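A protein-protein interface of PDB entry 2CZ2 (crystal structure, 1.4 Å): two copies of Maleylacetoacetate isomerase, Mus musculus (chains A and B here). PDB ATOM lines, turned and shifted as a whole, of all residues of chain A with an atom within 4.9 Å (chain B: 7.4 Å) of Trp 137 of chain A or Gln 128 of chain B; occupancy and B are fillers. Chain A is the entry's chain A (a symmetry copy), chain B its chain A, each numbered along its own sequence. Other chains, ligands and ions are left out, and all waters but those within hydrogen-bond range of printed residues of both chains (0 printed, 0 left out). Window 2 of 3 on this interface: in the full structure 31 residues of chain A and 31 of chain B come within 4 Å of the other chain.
O of Leu 120 of chain A sits at hydrogen-bond distance from NE1 of Trp 137 of chain A.
NE1 of Trp 137 of chain B lies within hydrogen-bond range of O of Leu 120 of chain B (2.8 Å).
Leu 120 of chain A touches Val 125 of chain B.
CG2 of Val 125 of chain A touches CD2 of Leu 120 of chain B, at 3.7 Å.
CG2 of Val 129 of chain A touches CH2 of Trp 137 of chain B, 3.8 Å away.
Gln 128 of chain B touches Trp 137 of chain A (CB to CZ3, 3.9 Å).
CH2 of Trp 137 of chain A touches CG2 of Val 129 of chain B (3.8 Å).
Lys 140 of chain A touches Gln 128 of chain B (CE to NE2, 3.2 Å).
Printed residues of chain B within 4 Å of Leu 120 of chain A: Val 125 (3.7 Å).
Printed residues of chain B within 4 Å of Val 125 of chain A: Leu 120.
Gln 134 of chain A touches none of the printed residues of chain B.
Of chain B, only Gln 128 and Val 129 come within 4 Å of Trp 137 of chain A.
Of the printed residues of chain A, Val 125 of chain B touches Leu 120.
Gln 128 of chain B touches just these residues of chain A: Trp 137 and Lys 140.
Of the printed residues of chain A, Val 129 of chain B touches Trp 137 (3.8 Å).
The nearest printed residue of chain A that does not touch Gln 128 of chain B is Val 141 of chain A (6.6 Å).
The nearest printed residue of chain A that does not touch Val 129 of chain B is Val 129 of chain A (6.6 Å).
Along chain B the printed residues that touch a printed residue of chain A span positions 120 to 137.
Along chain A the printed residues that touch a printed residue of chain B span positions 120 to 140.
Among the printed residues, no Asp or Glu carboxylate lies within 4 Å of a Lys or Arg side-chain nitrogen of the other chain.
Leu 120 of chain A touches Val 125 of chain B, and with the chains exchanged Val 125 of chain A touches Leu 120 of chain B.
Val 129 of chain A touches Trp 137 of chain B, and with the chains exchanged Trp 137 of chain A touches Val 129 of chain B.
Positions printed for both chains: 120, 125, 126, 129, 134 and 137.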
ATOM      1  N   LEU A 120      -3.930 -22.116   3.837  1.00  0.00           N
ATOM      2  CA  LEU A 120      -3.908 -20.727   3.496  1.00  0.00           C
ATOM      3  C   LEU A 120      -2.786 -20.427   2.516  1.00  0.00           C
ATOM      4  O   LEU A 120      -2.741 -19.324   1.986  1.00  0.00           O
ATOM      5  CB  LEU A 120      -3.777 -19.873   4.765  1.00  0.00           C
ATOM      6  CG  LEU A 120      -4.929 -19.771   5.776  1.00  0.00           C
ATOM      7  CD1 LEU A 120      -5.504 -21.099   6.233  1.00  0.00           C
ATOM      8  CD2 LEU A 120      -4.456 -19.031   6.998  1.00  0.00           C
ATOM      9  N   VAL A 125      -5.664 -21.444  -3.313  1.00  0.00           N
ATOM     10  CA  VAL A 125      -5.823 -20.209  -2.565  1.00  0.00           C
ATOM     11  C   VAL A 125      -4.901 -19.115  -3.105  1.00  0.00           C
ATOM     12  O   VAL A 125      -5.325 -17.986  -3.302  1.00  0.00           O
ATOM     13  CB  VAL A 125      -5.582 -20.451  -1.054  1.00  0.00           C
ATOM     14  CG1 VAL A 125      -5.573 -19.132  -0.283  1.00  0.00           C
ATOM     15  CG2 VAL A 125      -6.642 -21.369  -0.505  1.00  0.00           C
ATOM     16  N   LEU A 126      -3.633 -19.439  -3.331  1.00  0.00           N
ATOM     17  CA  LEU A 126      -2.700 -18.489  -3.923  1.00  0.00           C
ATOM     18  C   LEU A 126      -3.191 -18.004  -5.293  1.00  0.00           C
ATOM     19  O   LEU A 126      -3.047 -16.817  -5.601  1.00  0.00           O
ATOM     20  CB  LEU A 126      -1.297 -19.060  -4.004  1.00  0.00           C
ATOM     21  CG  LEU A 126      -0.700 -19.387  -2.626  1.00  0.00           C
ATOM     22  CD1 LEU A 126       0.761 -19.795  -2.701  1.00  0.00           C
ATOM     23  CD2 LEU A 126      -0.869 -18.230  -1.654  1.00  0.00           C
ATOM     24  N   VAL A 129      -5.719 -15.334  -4.608  1.00  0.00           N
ATOM     25  CA  VAL A 129      -5.070 -14.110  -4.131  1.00  0.00           C
ATOM     26  C   VAL A 129      -4.534 -13.287  -5.324  1.00  0.00           C
ATOM     27  O   VAL A 129      -4.627 -12.053  -5.365  1.00  0.00           O
ATOM     28  CB  VAL A 129      -3.913 -14.462  -3.157  1.00  0.00           C
ATOM     29  CG1 VAL A 129      -3.070 -13.230  -2.817  1.00  0.00           C
ATOM     30  CG2 VAL A 129      -4.476 -15.087  -1.906  1.00  0.00           C
ATOM     31  N   ASN A 133       0.062 -10.478  -5.225  1.00  0.00           N
ATOM     32  CA  ASN A 133       0.089 -10.579  -3.774  1.00  0.00           C
ATOM     33  C   ASN A 133       0.365 -11.975  -3.206  1.00  0.00           C
ATOM     34  O   ASN A 133       0.530 -12.099  -2.012  1.00  0.00           O
ATOM     35  CB  ASN A 133      -1.223 -10.025  -3.218  1.00  0.00           C
ATOM     36  CG  ASN A 133      -1.344  -8.521  -3.432  1.00  0.00           C
ATOM     37  OD1 ASN A 133      -0.397  -7.784  -3.168  1.00  0.00           O
ATOM     38  ND2 ASN A 133      -2.498  -8.067  -3.934  1.00  0.00           N
ATOM     39  N   GLN A 134       0.424 -13.014  -4.028  1.00  0.00           N
ATOM     40  CA  GLN A 134       0.478 -14.387  -3.462  1.00  0.00           C
ATOM     41  C   GLN A 134       1.722 -14.693  -2.631  1.00  0.00           C
ATOM     42  O   GLN A 134       1.649 -15.392  -1.629  1.00  0.00           O
ATOM     43  CB  GLN A 134       0.294 -15.474  -4.537  1.00  0.00           C
ATOM     44  CG  GLN A 134       1.246 -15.384  -5.734  1.00  0.00           C
ATOM     45  CD  GLN A 134       2.536 -16.190  -5.608  1.00  0.00           C
ATOM     46  OE1 GLN A 134       3.549 -15.847  -6.263  1.00  0.00           O
ATOM     47  NE2 GLN A 134       2.520 -17.249  -4.814  1.00  0.00           N
ATOM     48  N   MET A 135       2.875 -14.198  -3.054  1.00  0.00           N
ATOM     49  CA  MET A 135       4.096 -14.419  -2.318  1.00  0.00           C
ATOM     50  C   MET A 135       4.028 -13.854  -0.904  1.00  0.00           C
ATOM     51  O   MET A 135       4.305 -14.555   0.087  1.00  0.00           O
ATOM     52  CB  MET A 135       5.240 -13.762  -3.051  1.00  0.00           C
ATOM     53  CG  MET A 135       6.517 -13.938  -2.320  1.00  0.00           C
ATOM     54  SD  MET A 135       7.088 -15.793  -2.417  1.00  0.00           S
ATOM     55  CE  MET A 135       6.327 -16.363  -4.121  1.00  0.00           C
ATOM     56  N   GLN A 136       3.679 -12.579  -0.805  1.00  0.00           N
ATOM     57  CA  GLN A 136       3.560 -11.915   0.499  1.00  0.00           C
ATOM     58  C   GLN A 136       2.491 -12.573   1.379  1.00  0.00           C
ATOM     59  O   GLN A 136       2.658 -12.718   2.592  1.00  0.00           O
ATOM     60  CB  GLN A 136       3.249 -10.422   0.315  1.00  0.00           C
ATOM     61  CG  GLN A 136       2.917  -9.695   1.610  1.00  0.00           C
ATOM     62  CD  GLN A 136       3.040  -8.177   1.478  1.00  0.00           C
ATOM     63  OE1 GLN A 136       3.684  -7.531   2.305  1.00  0.00           O
ATOM     64  NE2 GLN A 136       2.442  -7.618   0.439  1.00  0.00           N
ATOM     65  N   TRP A 137       1.397 -12.987   0.754  1.00  0.00           N
ATOM     66  CA  TRP A 137       0.342 -13.697   1.458  1.00  0.00           C
ATOM     67  C   TRP A 137       0.879 -14.987   2.074  1.00  0.00           C
ATOM     68  O   TRP A 137       0.661 -15.281   3.262  1.00  0.00           O
ATOM     69  CB  TRP A 137      -0.777 -14.044   0.463  1.00  0.00           C
ATOM     70  CG  TRP A 137      -1.913 -14.878   1.020  1.00  0.00           C
ATOM     71  CD1 TRP A 137      -1.920 -16.224   1.258  1.00  0.00           C
ATOM     72  CD2 TRP A 137      -3.230 -14.415   1.340  1.00  0.00           C
ATOM     73  NE1 TRP A 137      -3.142 -16.606   1.744  1.00  0.00           N
ATOM     74  CE2 TRP A 137      -3.961 -15.515   1.811  1.00  0.00           C
ATOM     75  CE3 TRP A 137      -3.868 -13.169   1.270  1.00  0.00           C
ATOM     76  CZ2 TRP A 137      -5.293 -15.428   2.200  1.00  0.00           C
ATOM     77  CZ3 TRP A 137      -5.199 -13.071   1.701  1.00  0.00           C
ATOM     78  CH2 TRP A 137      -5.896 -14.204   2.151  1.00  0.00           C
ATOM     79  N   ALA A 138       1.565 -15.781   1.263  1.00  0.00           N
ATOM     80  CA  ALA A 138       2.090 -17.056   1.749  1.00  0.00           C
ATOM     81  C   ALA A 138       3.081 -16.830   2.895  1.00  0.00           C
ATOM     82  O   ALA A 138       3.106 -17.549   3.896  1.00  0.00           O
ATOM     83  CB  ALA A 138       2.771 -17.778   0.616  1.00  0.00           C
ATOM     84  N   GLN A 139       3.935 -15.831   2.738  1.00  0.00           N
ATOM     85  CA  GLN A 139       4.910 -15.509   3.767  1.00  0.00           C
ATOM     86  C   GLN A 139       4.245 -15.098   5.084  1.00  0.00           C
ATOM     87  O   GLN A 139       4.662 -15.502   6.152  1.00  0.00           O
ATOM     88  CB  GLN A 139       5.841 -14.413   3.268  1.00  0.00           C
ATOM     89  CG  GLN A 139       6.776 -14.890   2.156  1.00  0.00           C
ATOM     90  CD  GLN A 139       7.578 -13.752   1.551  1.00  0.00           C
ATOM     91  OE1 GLN A 139       7.148 -12.594   1.609  1.00  0.00           O
ATOM     92  NE2 GLN A 139       8.769 -14.068   1.016  1.00  0.00           N
ATOM     93  N   LYS A 140       3.193 -14.297   4.995  1.00  0.00           N
ATOM     94  CA  LYS A 140       2.458 -13.866   6.169  1.00  0.00           C
ATOM     95  C   LYS A 140       1.812 -15.053   6.902  1.00  0.00           C
ATOM     96  O   LYS A 140       1.913 -15.196   8.133  1.00  0.00           O
ATOM     97  CB  LYS A 140       1.436 -12.780   5.755  1.00  0.00           C
ATOM     98  CG  LYS A 140       0.476 -12.339   6.823  1.00  0.00           C
ATOM     99  CD  LYS A 140       1.144 -11.835   8.065  1.00  0.00           C
ATOM    100  CE  LYS A 140       0.164 -11.060   8.966  1.00  0.00           C
ATOM    101  NZ  LYS A 140       0.861 -10.020   9.778  1.00  0.00           N
ATOM    102  N   VAL A 141       1.162 -15.937   6.155  1.00  0.00           N
ATOM    103  CA  VAL A 141       0.516 -17.102   6.777  1.00  0.00           C
ATOM    104  C   VAL A 141       1.515 -18.009   7.467  1.00  0.00           C
ATOM    105  O   VAL A 141       1.248 -18.508   8.537  1.00  0.00           O
ATOM    106  CB  VAL A 141      -0.255 -17.877   5.720  1.00  0.00           C
ATOM    107  CG1 VAL A 141      -0.662 -19.272   6.211  1.00  0.00           C
ATOM    108  CG2 VAL A 141      -1.433 -16.938   5.270  1.00  0.00           C
ATOM    109  N   LEU B 120     -10.238 -20.994   5.480  1.00  0.00           N
ATOM    110  CA  LEU B 120     -10.220 -20.064   4.393  1.00  0.00           C
ATOM    111  C   LEU B 120     -11.319 -19.026   4.549  1.00  0.00           C
ATOM    112  O   LEU B 120     -11.327 -18.056   3.802  1.00  0.00           O
ATOM    113  CB  LEU B 120     -10.349 -20.810   3.059  1.00  0.00           C
ATOM    114  CG  LEU B 120      -9.212 -21.695   2.531  1.00  0.00           C
ATOM    115  CD1 LEU B 120      -8.677 -22.716   3.518  1.00  0.00           C
ATOM    116  CD2 LEU B 120      -9.684 -22.443   1.312  1.00  0.00           C
ATOM    117  N   ASN B 122     -12.076 -17.968   7.871  1.00  0.00           N
ATOM    118  CA  ASN B 122     -11.835 -17.495   9.217  1.00  0.00           C
ATOM    119  C   ASN B 122     -11.672 -15.971   9.223  1.00  0.00           C
ATOM    120  O   ASN B 122     -11.241 -15.374   8.224  1.00  0.00           O
ATOM    121  CB  ASN B 122     -10.592 -18.190   9.770  1.00  0.00           C
ATOM    122  CG  ASN B 122     -10.292 -17.838  11.215  1.00  0.00           C
ATOM    123  OD1 ASN B 122     -11.207 -17.694  12.054  1.00  0.00           O
ATOM    124  ND2 ASN B 122      -9.010 -17.752  11.535  1.00  0.00           N
ATOM    125  N   LEU B 123     -11.991 -15.355  10.363  1.00  0.00           N
ATOM    126  CA  LEU B 123     -11.978 -13.913  10.558  1.00  0.00           C
ATOM    127  C   LEU B 123     -10.665 -13.291  10.127  1.00  0.00           C
ATOM    128  O   LEU B 123     -10.661 -12.361   9.338  1.00  0.00           O
ATOM    129  CB  LEU B 123     -12.256 -13.612  12.040  1.00  0.00           C
ATOM    130  CG  LEU B 123     -12.212 -12.154  12.458  1.00  0.00           C
ATOM    131  CD1 LEU B 123     -13.265 -11.349  11.681  1.00  0.00           C
ATOM    132  CD2 LEU B 123     -12.421 -12.055  13.961  1.00  0.00           C
ATOM    133  N   SER B 124      -9.550 -13.811  10.622  1.00  0.00           N
ATOM    134  CA  SER B 124      -8.251 -13.237  10.301  1.00  0.00           C
ATOM    135  C   SER B 124      -7.926 -13.309   8.803  1.00  0.00           C
ATOM    136  O   SER B 124      -7.265 -12.425   8.278  1.00  0.00           O
ATOM    137  CB  SER B 124      -7.120 -13.892  11.081  1.00  0.00           C
ATOM    138  OG  SER B 124      -7.019 -15.272  10.783  1.00  0.00           O
ATOM    139  N   VAL B 125      -8.377 -14.352   8.125  1.00  0.00           N
ATOM    140  CA  VAL B 125      -8.198 -14.468   6.688  1.00  0.00           C
ATOM    141  C   VAL B 125      -9.085 -13.470   5.941  1.00  0.00           C
ATOM    142  O   VAL B 125      -8.629 -12.798   5.028  1.00  0.00           O
ATOM    143  CB  VAL B 125      -8.470 -15.919   6.221  1.00  0.00           C
ATOM    144  CG1 VAL B 125      -8.457 -16.014   4.696  1.00  0.00           C
ATOM    145  CG2 VAL B 125      -7.442 -16.849   6.810  1.00  0.00           C
ATOM    146  N   LEU B 126     -10.357 -13.382   6.313  1.00  0.00           N
ATOM    147  CA  LEU B 126     -11.256 -12.404   5.716  1.00  0.00           C
ATOM    148  C   LEU B 126     -10.732 -10.974   5.907  1.00  0.00           C
ATOM    149  O   LEU B 126     -10.841 -10.162   4.983  1.00  0.00           O
ATOM    150  CB  LEU B 126     -12.672 -12.551   6.240  1.00  0.00           C
ATOM    151  CG  LEU B 126     -13.298 -13.915   5.902  1.00  0.00           C
ATOM    152  CD1 LEU B 126     -14.767 -13.994   6.278  1.00  0.00           C
ATOM    153  CD2 LEU B 126     -13.115 -14.267   4.435  1.00  0.00           C
ATOM    154  N   LYS B 127     -10.074 -10.694   7.039  1.00  0.00           N
ATOM    155  CA  LYS B 127      -9.490  -9.361   7.262  1.00  0.00           C
ATOM    156  C   LYS B 127      -8.364  -9.080   6.274  1.00  0.00           C
ATOM    157  O   LYS B 127      -8.242  -7.949   5.753  1.00  0.00           O
ATOM    158  CB  LYS B 127      -9.024  -9.202   8.719  1.00  0.00           C
ATOM    159  CG  LYS B 127     -10.199  -9.164   9.706  1.00  0.00           C
ATOM    160  CD  LYS B 127     -10.659  -7.759  10.033  1.00  0.00           C
ATOM    161  CE  LYS B 127     -11.772  -7.760  11.095  1.00  0.00           C
ATOM    162  NZ  LYS B 127     -11.264  -8.007  12.487  1.00  0.00           N
ATOM    163  N   GLN B 128      -7.540 -10.082   6.010  1.00  0.00           N
ATOM    164  CA  GLN B 128      -6.485  -9.959   4.994  1.00  0.00           C
ATOM    165  C   GLN B 128      -7.002  -9.841   3.554  1.00  0.00           C
ATOM    166  O   GLN B 128      -6.380  -9.201   2.724  1.00  0.00           O
ATOM    167  CB  GLN B 128      -5.511 -11.127   5.106  1.00  0.00           C
ATOM    168  CG  GLN B 128      -4.784 -11.156   6.424  1.00  0.00           C
ATOM    169  CD  GLN B 128      -3.510 -10.319   6.434  1.00  0.00           C
ATOM    170  OE1 GLN B 128      -3.344  -9.386   5.630  1.00  0.00           O
ATOM    171  NE2 GLN B 128      -2.601 -10.656   7.347  1.00  0.00           N
ATOM    172  N   VAL B 129      -8.147 -10.449   3.254  1.00  0.00           N
ATOM    173  CA  VAL B 129      -8.774 -10.309   1.936  1.00  0.00           C
ATOM    174  C   VAL B 129      -9.270  -8.859   1.730  1.00  0.00           C
ATOM    175  O   VAL B 129      -9.146  -8.271   0.649  1.00  0.00           O
ATOM    176  CB  VAL B 129      -9.954 -11.307   1.794  1.00  0.00           C
ATOM    177  CG1 VAL B 129     -10.771 -11.035   0.529  1.00  0.00           C
ATOM    178  CG2 VAL B 129      -9.427 -12.719   1.797  1.00  0.00           C
ATOM    179  N   GLY B 130      -9.817  -8.287   2.792  1.00  0.00           N
ATOM    180  CA  GLY B 130     -10.307  -6.923   2.777  1.00  0.00           C
ATOM    181  C   GLY B 130     -11.812  -6.837   2.654  1.00  0.00           C
ATOM    182  O   GLY B 130     -12.465  -7.760   2.181  1.00  0.00           O
ATOM    183  N   GLN B 131     -12.359  -5.705   3.078  1.00  0.00           N
ATOM    184  CA  GLN B 131     -13.806  -5.500   3.098  1.00  0.00           C
ATOM    185  C   GLN B 131     -14.449  -5.701   1.721  1.00  0.00           C
ATOM    186  O   GLN B 131     -15.519  -6.277   1.637  1.00  0.00           O
ATOM    187  CB  GLN B 131     -14.140  -4.097   3.651  1.00  0.00           C
ATOM    188  CG  GLN B 131     -15.376  -4.032   4.568  1.00  0.00           C
ATOM    189  CD  GLN B 131     -15.443  -2.742   5.421  1.00  0.00           C
ATOM    190  OE1 GLN B 131     -16.150  -1.783   5.064  1.00  0.00           O
ATOM    191  NE2 GLN B 131     -14.714  -2.723   6.540  1.00  0.00           N
ATOM    192  N   GLN B 134     -14.239  -9.769   0.826  1.00  0.00           N
ATOM    193  CA  GLN B 134     -14.337 -10.890   1.796  1.00  0.00           C
ATOM    194  C   GLN B 134     -15.600 -11.739   1.675  1.00  0.00           C
ATOM    195  O   GLN B 134     -15.561 -12.949   1.851  1.00  0.00           O
ATOM    196  CB  GLN B 134     -14.163 -10.425   3.253  1.00  0.00           C
ATOM    197  CG  GLN B 134     -15.094  -9.291   3.697  1.00  0.00           C
ATOM    198  CD  GLN B 134     -16.406  -9.733   4.339  1.00  0.00           C
ATOM    199  OE1 GLN B 134     -17.399  -8.969   4.312  1.00  0.00           O
ATOM    200  NE2 GLN B 134     -16.429 -10.918   4.928  1.00  0.00           N
ATOM    201  N   TRP B 137     -15.285 -14.002  -1.365  1.00  0.00           N
ATOM    202  CA  TRP B 137     -14.259 -14.977  -1.031  1.00  0.00           C
ATOM    203  C   TRP B 137     -14.838 -16.093  -0.165  1.00  0.00           C
ATOM    204  O   TRP B 137     -14.646 -17.291  -0.434  1.00  0.00           O
ATOM    205  CB  TRP B 137     -13.134 -14.273  -0.257  1.00  0.00           C
ATOM    206  CG  TRP B 137     -12.028 -15.174   0.255  1.00  0.00           C
ATOM    207  CD1 TRP B 137     -12.059 -15.991   1.349  1.00  0.00           C
ATOM    208  CD2 TRP B 137     -10.705 -15.284  -0.283  1.00  0.00           C
ATOM    209  NE1 TRP B 137     -10.855 -16.628   1.491  1.00  0.00           N
ATOM    210  CE2 TRP B 137     -10.009 -16.218   0.498  1.00  0.00           C
ATOM    211  CE3 TRP B 137     -10.035 -14.678  -1.353  1.00  0.00           C
ATOM    212  CZ2 TRP B 137      -8.682 -16.560   0.267  1.00  0.00           C
ATOM    213  CZ3 TRP B 137      -8.709 -15.051  -1.614  1.00  0.00           C
ATOM    214  CH2 TRP B 137      -8.048 -15.981  -0.794  1.00  0.00           C
